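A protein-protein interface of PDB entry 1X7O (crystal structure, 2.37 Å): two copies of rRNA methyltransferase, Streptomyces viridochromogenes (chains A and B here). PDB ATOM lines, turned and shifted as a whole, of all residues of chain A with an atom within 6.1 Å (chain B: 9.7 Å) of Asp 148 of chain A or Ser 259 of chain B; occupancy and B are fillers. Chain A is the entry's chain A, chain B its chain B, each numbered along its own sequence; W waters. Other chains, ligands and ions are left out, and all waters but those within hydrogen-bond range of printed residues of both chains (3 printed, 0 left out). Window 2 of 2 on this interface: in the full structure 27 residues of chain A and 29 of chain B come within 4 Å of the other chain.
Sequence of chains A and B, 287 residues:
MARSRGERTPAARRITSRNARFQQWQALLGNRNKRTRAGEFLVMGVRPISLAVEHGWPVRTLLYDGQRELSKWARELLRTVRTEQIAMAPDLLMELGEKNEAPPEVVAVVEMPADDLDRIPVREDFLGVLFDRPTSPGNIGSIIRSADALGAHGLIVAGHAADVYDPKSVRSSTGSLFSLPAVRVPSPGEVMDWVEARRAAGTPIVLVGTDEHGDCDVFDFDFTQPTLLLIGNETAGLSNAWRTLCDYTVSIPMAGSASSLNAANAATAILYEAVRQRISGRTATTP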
ATOM      1  N   ARG A  47      38.526  20.454  35.462  1.00  0.00           N
ATOM      2  CA  ARG A  47      37.896  20.021  34.226  1.00  0.00           C
ATOM      3  C   ARG A  47      37.552  21.204  33.353  1.00  0.00           C
ATOM      4  O   ARG A  47      37.960  21.200  32.202  1.00  0.00           O
ATOM      5  CB  ARG A  47      36.692  19.104  34.455  1.00  0.00           C
ATOM      6  CG  ARG A  47      36.231  18.434  33.173  1.00  0.00           C
ATOM      7  CD  ARG A  47      34.922  17.688  33.283  1.00  0.00           C
ATOM      8  NE  ARG A  47      34.461  17.221  31.968  1.00  0.00           N
ATOM      9  CZ  ARG A  47      33.538  17.825  31.207  1.00  0.00           C
ATOM     10  NH1 ARG A  47      32.957  18.964  31.596  1.00  0.00           N
ATOM     11  NH2 ARG A  47      33.200  17.297  30.030  1.00  0.00           N
ATOM     12  N   ILE A 143      21.362  26.243  28.874  1.00  0.00           N
ATOM     13  CA  ILE A 143      21.106  26.360  27.435  1.00  0.00           C
ATOM     14  C   ILE A 143      22.388  26.221  26.657  1.00  0.00           C
ATOM     15  O   ILE A 143      22.383  25.572  25.619  1.00  0.00           O
ATOM     16  CB  ILE A 143      20.360  27.683  27.057  1.00  0.00           C
ATOM     17  CG1 ILE A 143      18.929  27.622  27.569  1.00  0.00           C
ATOM     18  CG2 ILE A 143      20.314  27.875  25.517  1.00  0.00           C
ATOM     19  CD1 ILE A 143      18.134  28.866  27.328  1.00  0.00           C
ATOM     20  N   ILE A 144      23.490  26.804  27.150  1.00  0.00           N
ATOM     21  CA  ILE A 144      24.789  26.662  26.471  1.00  0.00           C
ATOM     22  C   ILE A 144      25.126  25.183  26.390  1.00  0.00           C
ATOM     23  O   ILE A 144      25.557  24.693  25.349  1.00  0.00           O
ATOM     24  CB  ILE A 144      25.928  27.436  27.188  1.00  0.00           C
ATOM     25  CG1 ILE A 144      25.798  28.954  26.968  1.00  0.00           C
ATOM     26  CG2 ILE A 144      27.288  27.001  26.662  1.00  0.00           C
ATOM     27  CD1 ILE A 144      26.790  29.780  27.774  1.00  0.00           C
ATOM     28  N   ARG A 145      24.883  24.460  27.478  1.00  0.00           N
ATOM     29  CA  ARG A 145      25.192  23.036  27.539  1.00  0.00           C
ATOM     30  C   ARG A 145      24.346  22.202  26.566  1.00  0.00           C
ATOM     31  O   ARG A 145      24.885  21.356  25.837  1.00  0.00           O
ATOM     32  CB  ARG A 145      25.019  22.545  28.980  1.00  0.00           C
ATOM     33  CG  ARG A 145      25.146  21.067  29.170  1.00  0.00           C
ATOM     34  CD  ARG A 145      25.039  20.654  30.607  1.00  0.00           C
ATOM     35  NE  ARG A 145      25.477  19.285  30.824  1.00  0.00           N
ATOM     36  CZ  ARG A 145      25.475  18.682  32.010  1.00  0.00           C
ATOM     37  NH1 ARG A 145      25.056  19.312  33.099  1.00  0.00           N
ATOM     38  NH2 ARG A 145      25.895  17.438  32.110  1.00  0.00           N
ATOM     39  N   SER A 146      23.034  22.432  26.555  1.00  0.00           N
ATOM     40  CA  SER A 146      22.144  21.750  25.623  1.00  0.00           C
ATOM     41  C   SER A 146      22.447  22.087  24.161  1.00  0.00           C
ATOM     42  O   SER A 146      22.452  21.207  23.320  1.00  0.00           O
ATOM     43  CB  SER A 146      20.686  22.076  25.940  1.00  0.00           C
ATOM     44  OG  SER A 146      20.324  21.459  27.153  1.00  0.00           O
ATOM     45  N   ALA A 147      22.707  23.352  23.867  1.00  0.00           N
ATOM     46  CA  ALA A 147      22.963  23.773  22.492  1.00  0.00           C
ATOM     47  C   ALA A 147      24.226  23.118  21.961  1.00  0.00           C
ATOM     48  O   ALA A 147      24.268  22.657  20.801  1.00  0.00           O
ATOM     49  CB  ALA A 147      23.065  25.302  22.408  1.00  0.00           C
ATOM     50  N   ASP A 148      25.239  23.060  22.838  1.00  0.00           N
ATOM     51  CA  ASP A 148      26.505  22.392  22.568  1.00  0.00           C
ATOM     52  C   ASP A 148      26.268  20.923  22.261  1.00  0.00           C
ATOM     53  O   ASP A 148      26.727  20.404  21.223  1.00  0.00           O
ATOM     54  CB  ASP A 148      27.413  22.523  23.792  1.00  0.00           C
ATOM     55  CG  ASP A 148      28.761  21.885  23.599  1.00  0.00           C
ATOM     56  OD1 ASP A 148      29.404  22.088  22.550  1.00  0.00           O
ATOM     57  OD2 ASP A 148      29.281  21.163  24.465  1.00  0.00           O
ATOM     58  N   ALA A 149      25.522  20.258  23.151  1.00  0.00           N
ATOM     59  CA  ALA A 149      25.322  18.815  23.065  1.00  0.00           C
ATOM     60  C   ALA A 149      24.468  18.438  21.877  1.00  0.00           C
ATOM     61  O   ALA A 149      24.623  17.369  21.332  1.00  0.00           O
ATOM     62  CB  ALA A 149      24.688  18.281  24.341  1.00  0.00           C
ATOM     63  N   LEU A 150      23.562  19.314  21.468  1.00  0.00           N
ATOM     64  CA  LEU A 150      22.589  18.953  20.440  1.00  0.00           C
ATOM     65  C   LEU A 150      22.913  19.517  19.051  1.00  0.00           C
ATOM     66  O   LEU A 150      22.077  19.446  18.152  1.00  0.00           O
ATOM     67  CB  LEU A 150      21.186  19.381  20.884  1.00  0.00           C
ATOM     68  CG  LEU A 150      20.652  18.543  22.053  1.00  0.00           C
ATOM     69  CD1 LEU A 150      19.453  19.218  22.652  1.00  0.00           C
ATOM     70  CD2 LEU A 150      20.288  17.135  21.602  1.00  0.00           C
ATOM     71  N   GLY A 151      24.114  20.065  18.876  1.00  0.00           N
ATOM     72  CA  GLY A 151      24.597  20.496  17.572  1.00  0.00           C
ATOM     73  C   GLY A 151      24.301  21.922  17.131  1.00  0.00           C
ATOM     74  O   GLY A 151      24.581  22.253  16.005  1.00  0.00           O
ATOM     75  N   ALA A 152      23.716  22.768  17.976  1.00  0.00           N
ATOM     76  CA  ALA A 152      23.613  24.198  17.664  1.00  0.00           C
ATOM     77  C   ALA A 152      25.012  24.794  17.506  1.00  0.00           C
ATOM     78  O   ALA A 152      25.987  24.222  17.996  1.00  0.00           O
ATOM     79  CB  ALA A 152      22.820  24.946  18.740  1.00  0.00           C
ATOM     80  N   GLY A 175      31.466  23.364  31.295  1.00  0.00           N
ATOM     81  CA  GLY A 175      32.588  23.411  30.376  1.00  0.00           C
ATOM     82  C   GLY A 175      32.201  23.680  28.929  1.00  0.00           C
ATOM     83  O   GLY A 175      33.071  23.922  28.115  1.00  0.00           O
ATOM     84  N   SER A 176      30.909  23.637  28.614  1.00  0.00           N
ATOM     85  CA  SER A 176      30.435  23.843  27.238  1.00  0.00           C
ATOM     86  C   SER A 176      30.577  25.269  26.742  1.00  0.00           C
ATOM     87  O   SER A 176      30.572  25.503  25.529  1.00  0.00           O
ATOM     88  CB  SER A 176      28.963  23.414  27.109  1.00  0.00           C
ATOM     89  OG  SER A 176      28.938  22.007  26.973  1.00  0.00           O
ATOM     90  N   SER A 179      33.424  25.531  24.196  1.00  0.00           N
ATOM     91  CA  SER A 179      33.293  24.988  22.830  1.00  0.00           C
ATOM     92  C   SER A 179      32.153  25.592  22.006  1.00  0.00           C
ATOM     93  O   SER A 179      32.166  25.484  20.801  1.00  0.00           O
ATOM     94  CB  SER A 179      33.177  23.454  22.850  1.00  0.00           C
ATOM     95  OG  SER A 179      32.152  23.026  23.715  1.00  0.00           O
ATOM     96  N   LEU A 180      31.196  26.245  22.655  1.00  0.00           N
ATOM     97  CA  LEU A 180      30.011  26.807  22.002  1.00  0.00           C
ATOM     98  C   LEU A 180      30.136  28.321  22.076  1.00  0.00           C
ATOM     99  O   LEU A 180      30.060  28.882  23.170  1.00  0.00           O
ATOM    100  CB  LEU A 180      28.741  26.371  22.755  1.00  0.00           C
ATOM    101  CG  LEU A 180      27.311  26.337  22.181  1.00  0.00           C
ATOM    102  CD1 LEU A 180      26.516  27.571  22.500  1.00  0.00           C
ATOM    103  CD2 LEU A 180      27.253  26.049  20.696  1.00  0.00           C
ATOM    104  N   ASP B 211      20.547   6.379  28.942  1.00  0.00           N
ATOM    105  CA  ASP B 211      21.933   5.935  29.004  1.00  0.00           C
ATOM    106  C   ASP B 211      22.893   6.817  28.217  1.00  0.00           C
ATOM    107  O   ASP B 211      22.497   7.545  27.304  1.00  0.00           O
ATOM    108  CB  ASP B 211      22.036   4.497  28.471  1.00  0.00           C
ATOM    109  CG  ASP B 211      22.631   3.527  29.486  1.00  0.00           C
ATOM    110  OD1 ASP B 211      22.102   3.468  30.619  1.00  0.00           O
ATOM    111  OD2 ASP B 211      23.609   2.780  29.245  1.00  0.00           O
ATOM    112  N   GLU B 212      24.166   6.720  28.592  1.00  0.00           N
ATOM    113  CA  GLU B 212      25.270   7.199  27.770  1.00  0.00           C
ATOM    114  C   GLU B 212      25.515   6.143  26.669  1.00  0.00           C
ATOM    115  O   GLU B 212      26.074   6.456  25.608  1.00  0.00           O
ATOM    116  CB  GLU B 212      26.577   7.401  28.587  1.00  0.00           C
ATOM    117  CG  GLU B 212      26.472   7.842  30.059  1.00  0.00           C
ATOM    118  CD  GLU B 212      27.668   7.405  30.918  1.00  0.00           C
ATOM    119  OE1 GLU B 212      27.659   7.650  32.150  1.00  0.00           O
ATOM    120  OE2 GLU B 212      28.625   6.813  30.380  1.00  0.00           O
ATOM    121  N   ILE B 252      19.340  10.086  23.772  1.00  0.00           N
ATOM    122  CA  ILE B 252      19.221  11.268  22.927  1.00  0.00           C
ATOM    123  C   ILE B 252      20.520  11.385  22.130  1.00  0.00           C
ATOM    124  O   ILE B 252      21.595  11.410  22.725  1.00  0.00           O
ATOM    125  CB  ILE B 252      19.043  12.518  23.783  1.00  0.00           C
ATOM    126  CG1 ILE B 252      17.818  12.385  24.682  1.00  0.00           C
ATOM    127  CG2 ILE B 252      18.912  13.766  22.888  1.00  0.00           C
ATOM    128  CD1 ILE B 252      17.790  13.364  25.825  1.00  0.00           C
ATOM    129  N   PRO B 253      20.443  11.485  20.805  1.00  0.00           N
ATOM    130  CA  PRO B 253      21.647  11.564  19.981  1.00  0.00           C
ATOM    131  C   PRO B 253      22.382  12.877  20.194  1.00  0.00           C
ATOM    132  O   PRO B 253      21.757  13.946  20.233  1.00  0.00           O
ATOM    133  CB  PRO B 253      21.110  11.457  18.554  1.00  0.00           C
ATOM    134  CG  PRO B 253      19.745  11.918  18.623  1.00  0.00           C
ATOM    135  CD  PRO B 253      19.218  11.584  19.993  1.00  0.00           C
ATOM    136  N   MET B 254      23.702  12.784  20.340  1.00  0.00           N
ATOM    137  CA  MET B 254      24.517  13.911  20.789  1.00  0.00           C
ATOM    138  C   MET B 254      25.519  14.296  19.709  1.00  0.00           C
ATOM    139  O   MET B 254      25.780  13.532  18.785  1.00  0.00           O
ATOM    140  CB  MET B 254      25.228  13.558  22.108  1.00  0.00           C
ATOM    141  CG  MET B 254      25.171  14.650  23.203  1.00  0.00           C
ATOM    142  SD  MET B 254      24.143  14.289  24.626  1.00  0.00           S
ATOM    143  CE  MET B 254      22.611  14.351  23.878  1.00  0.00           C
ATOM    144  N   ALA B 255      26.080  15.490  19.830  1.00  0.00           N
ATOM    145  CA  ALA B 255      26.945  16.042  18.787  1.00  0.00           C
ATOM    146  C   ALA B 255      28.305  15.356  18.761  1.00  0.00           C
ATOM    147  O   ALA B 255      28.956  15.303  17.714  1.00  0.00           O
ATOM    148  CB  ALA B 255      27.108  17.561  18.959  1.00  0.00           C
ATOM    149  N   GLY B 256      28.737  14.814  19.896  1.00  0.00           N
ATOM    150  CA  GLY B 256      30.062  14.222  19.956  1.00  0.00           C
ATOM    151  C   GLY B 256      30.538  13.758  21.319  1.00  0.00           C
ATOM    152  O   GLY B 256      29.746  13.525  22.241  1.00  0.00           O
ATOM    153  N   SER B 257      31.859  13.664  21.429  1.00  0.00           N
ATOM    154  CA  SER B 257      32.542  13.028  22.556  1.00  0.00           C
ATOM    155  C   SER B 257      32.112  13.516  23.954  1.00  0.00           C
ATOM    156  O   SER B 257      31.409  12.793  24.668  1.00  0.00           O
ATOM    157  CB  SER B 257      34.062  13.173  22.375  1.00  0.00           C
ATOM    158  OG  SER B 257      34.764  12.292  23.226  1.00  0.00           O
ATOM    159  N   ALA B 258      32.516  14.732  24.329  1.00  0.00           N
ATOM    160  CA  ALA B 258      32.401  15.206  25.714  1.00  0.00           C
ATOM    161  C   ALA B 258      31.151  16.047  25.970  1.00  0.00           C
ATOM    162  O   ALA B 258      31.212  17.060  26.669  1.00  0.00           O
ATOM    163  CB  ALA B 258      33.669  15.999  26.106  1.00  0.00           C
ATOM    164  N   SER B 259      30.010  15.619  25.431  1.00  0.00           N
ATOM    165  CA  SER B 259      28.763  16.345  25.648  1.00  0.00           C
ATOM    166  C   SER B 259      27.702  15.494  26.310  1.00  0.00           C
ATOM    167  O   SER B 259      27.432  14.371  25.892  1.00  0.00           O
ATOM    168  CB  SER B 259      28.226  16.894  24.331  1.00  0.00           C
ATOM    169  OG  SER B 259      29.057  17.952  23.865  1.00  0.00           O
ATOM    170  N   SER B 260      27.084  16.067  27.334  1.00  0.00           N
ATOM    171  CA  SER B 260      25.974  15.445  28.049  1.00  0.00           C
ATOM    172  C   SER B 260      24.913  16.490  28.372  1.00  0.00           C
ATOM    173  O   SER B 260      25.149  17.692  28.231  1.00  0.00           O
ATOM    174  CB  SER B 260      26.483  14.826  29.350  1.00  0.00           C
ATOM    175  OG  SER B 260      27.431  15.688  29.957  1.00  0.00           O
ATOM    176  N   LEU B 261      23.750  16.014  28.812  1.00  0.00           N
ATOM    177  CA  LEU B 261      22.646  16.867  29.211  1.00  0.00           C
ATOM    178  C   LEU B 261      22.415  16.773  30.715  1.00  0.00           C
ATOM    179  O   LEU B 261      22.512  15.693  31.296  1.00  0.00           O
ATOM    180  CB  LEU B 261      21.368  16.442  28.500  1.00  0.00           C
ATOM    181  CG  LEU B 261      21.226  16.724  27.003  1.00  0.00           C
ATOM    182  CD1 LEU B 261      19.874  16.200  26.533  1.00  0.00           C
ATOM    183  CD2 LEU B 261      21.387  18.209  26.658  1.00  0.00           C
ATOM    184  N   ASN B 262      22.124  17.917  31.334  1.00  0.00           N
ATOM    185  CA  ASN B 262      21.553  17.974  32.670  1.00  0.00           C
ATOM    186  C   ASN B 262      20.292  17.076  32.726  1.00  0.00           C
ATOM    187  O   ASN B 262      19.509  17.000  31.758  1.00  0.00           O
ATOM    188  CB  ASN B 262      21.269  19.453  33.031  1.00  0.00           C
ATOM    189  CG  ASN B 262      20.193  19.634  34.095  1.00  0.00           C
ATOM    190  OD1 ASN B 262      20.484  19.875  35.276  1.00  0.00           O
ATOM    191  ND2 ASN B 262      18.949  19.584  33.673  1.00  0.00           N
HETATM  192  O   HOH W   1      27.283  19.867  26.107  1.00  0.00           O
HETATM  193  O   HOH W   2      30.042  16.853  29.047  1.00  0.00           O
HETATM  194  O   HOH W   3      21.717  20.266  29.639  1.00  0.00           O
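The guanidinium group (NE) of Arg 145 of chain A sits at hydrogen-bond distance from the backbone carbonyl oxygen (O) of Ser 260 of chain B, 3.1 Å away.
The side-chain hydroxyl (OG) of Ser 259 of chain B lies within hydrogen-bond range of the side-chain carboxylate (OD2) of Asp 148 of chain A (3.3 Å).
The backbone NH (N) of Ala 255 of chain B lies within hydrogen-bond range of the backbone carbonyl oxygen (O) of Ala 149 of chain A (2.8 Å).
OD2 of Asp 148 of chain A sits at hydrogen-bond distance from OG of Ser 176 of chain A, 2.7 Å away.
The side-chain carboxylate (OD1) of Asp 148 of chain A sits at hydrogen-bond distance from the side-chain hydroxyl (OG) of Ser 179 of chain A, 3.1 Å away.
Ala 258 of chain B touches Arg 47 of chain A.
Arg 145 of chain A touches Leu 261 of chain B (NH2 to C, 3.8 Å).
Arg 145 of chain A touches Asn 262 of chain B.
Leu 261 of chain B touches Ser 146 of chain A.
O of Asp 148 of chain A touches CB of Ala 255 of chain B (3.7 Å).
Ala 149 of chain A touches Met 254 of chain B (O to CG, 3.3 Å).
Ala 149 of chain A touches Ser 259 of chain B.
Ser 260 of chain B touches Ala 149 of chain A.
CG2 of Ile 252 of chain B touches CD2 of Leu 150 of chain A (3.9 Å).
Gly 151 of chain A touches Ala 255 of chain B (N to CB, 3.9 Å).
Of the printed residues of chain B, Arg 47 of chain A touches Ala 258 (3.9 Å).
No residue of chain B comes within 4 Å of Ala 147 of chain A.
Of chain B, only Ala 255 and Ser 259 come within 4 Å of Asp 148 of chain A.
Ala 149 of chain A touches just these residues of chain B: Met 254 (3.3 Å), Ala 255 (2.8 Å), Ser 259 (3.7 Å) and Ser 260 (3.96 Å).
Of the printed residues of chain B, Leu 150 of chain A touches Ile 252 and Pro 253.
No residue of chain B comes within 4 Å of Ala 152 of chain A.
No residue of chain B comes within 4 Å of Ser 176 of chain A.
No residue of chain B comes within 4 Å of Ser 179 of chain A.
Glu 212 of chain B touches none of the printed residues of chain A.
Of the printed residues of chain A, Pro 253 of chain B touches Leu 150 (3.8 Å).
Of the printed residues of chain A, Met 254 of chain B touches Ala 149 (3.3 Å).
Of the printed residues of chain A, Ala 255 of chain B touches Asp 148 (3.7 Å), Ala 149 (2.8 Å) and Gly 151 (3.9 Å).
Ser 259 of chain B touches two residues of chain A.
Printed residues of chain B that touch a printed residue of chain A: Ile 252, Pro 253, Met 254, Ala 255, Ala 258, Ser 259, Ser 260, Leu 261 and Asn 262.
Hydrophobic or aromatic side chains of chain A within 4 Å of the printed part of chain B: Ala 149 and Leu 150.
Along chain A the printed residues that touch a printed residue of chain B span positions 47 to 151.
No position is printed for both chains.
Of the 14 pairs that touch across the chains among the printed residues, none has its exchanged pair printed and touching as well.
Water W2 lies within hydrogen-bond range of the backbone carbonyl oxygen (O) of Ala 258 of chain B (2.7 Å), the side-chain hydroxyl (OG) of Ser 260 of chain B (3.0 Å) and the guanidinium group (NH2) of Arg 47 of chain A (3.3 Å).
Water W1 lies within hydrogen-bond range of O of Arg 145 of chain A (2.8 Å), OG of Ser 176 of chain A (2.8 Å), OD2 of Asp 148 of chain A (2.9 Å), OG of Ser 259 of chain B (3.4 Å) and N of Ala 149 of chain A (3.5 Å).
Water W3 lies within hydrogen-bond range of N of Asn 262 of chain B (2.9 Å) and OG of Ser 146 of chain A (3.1 Å).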
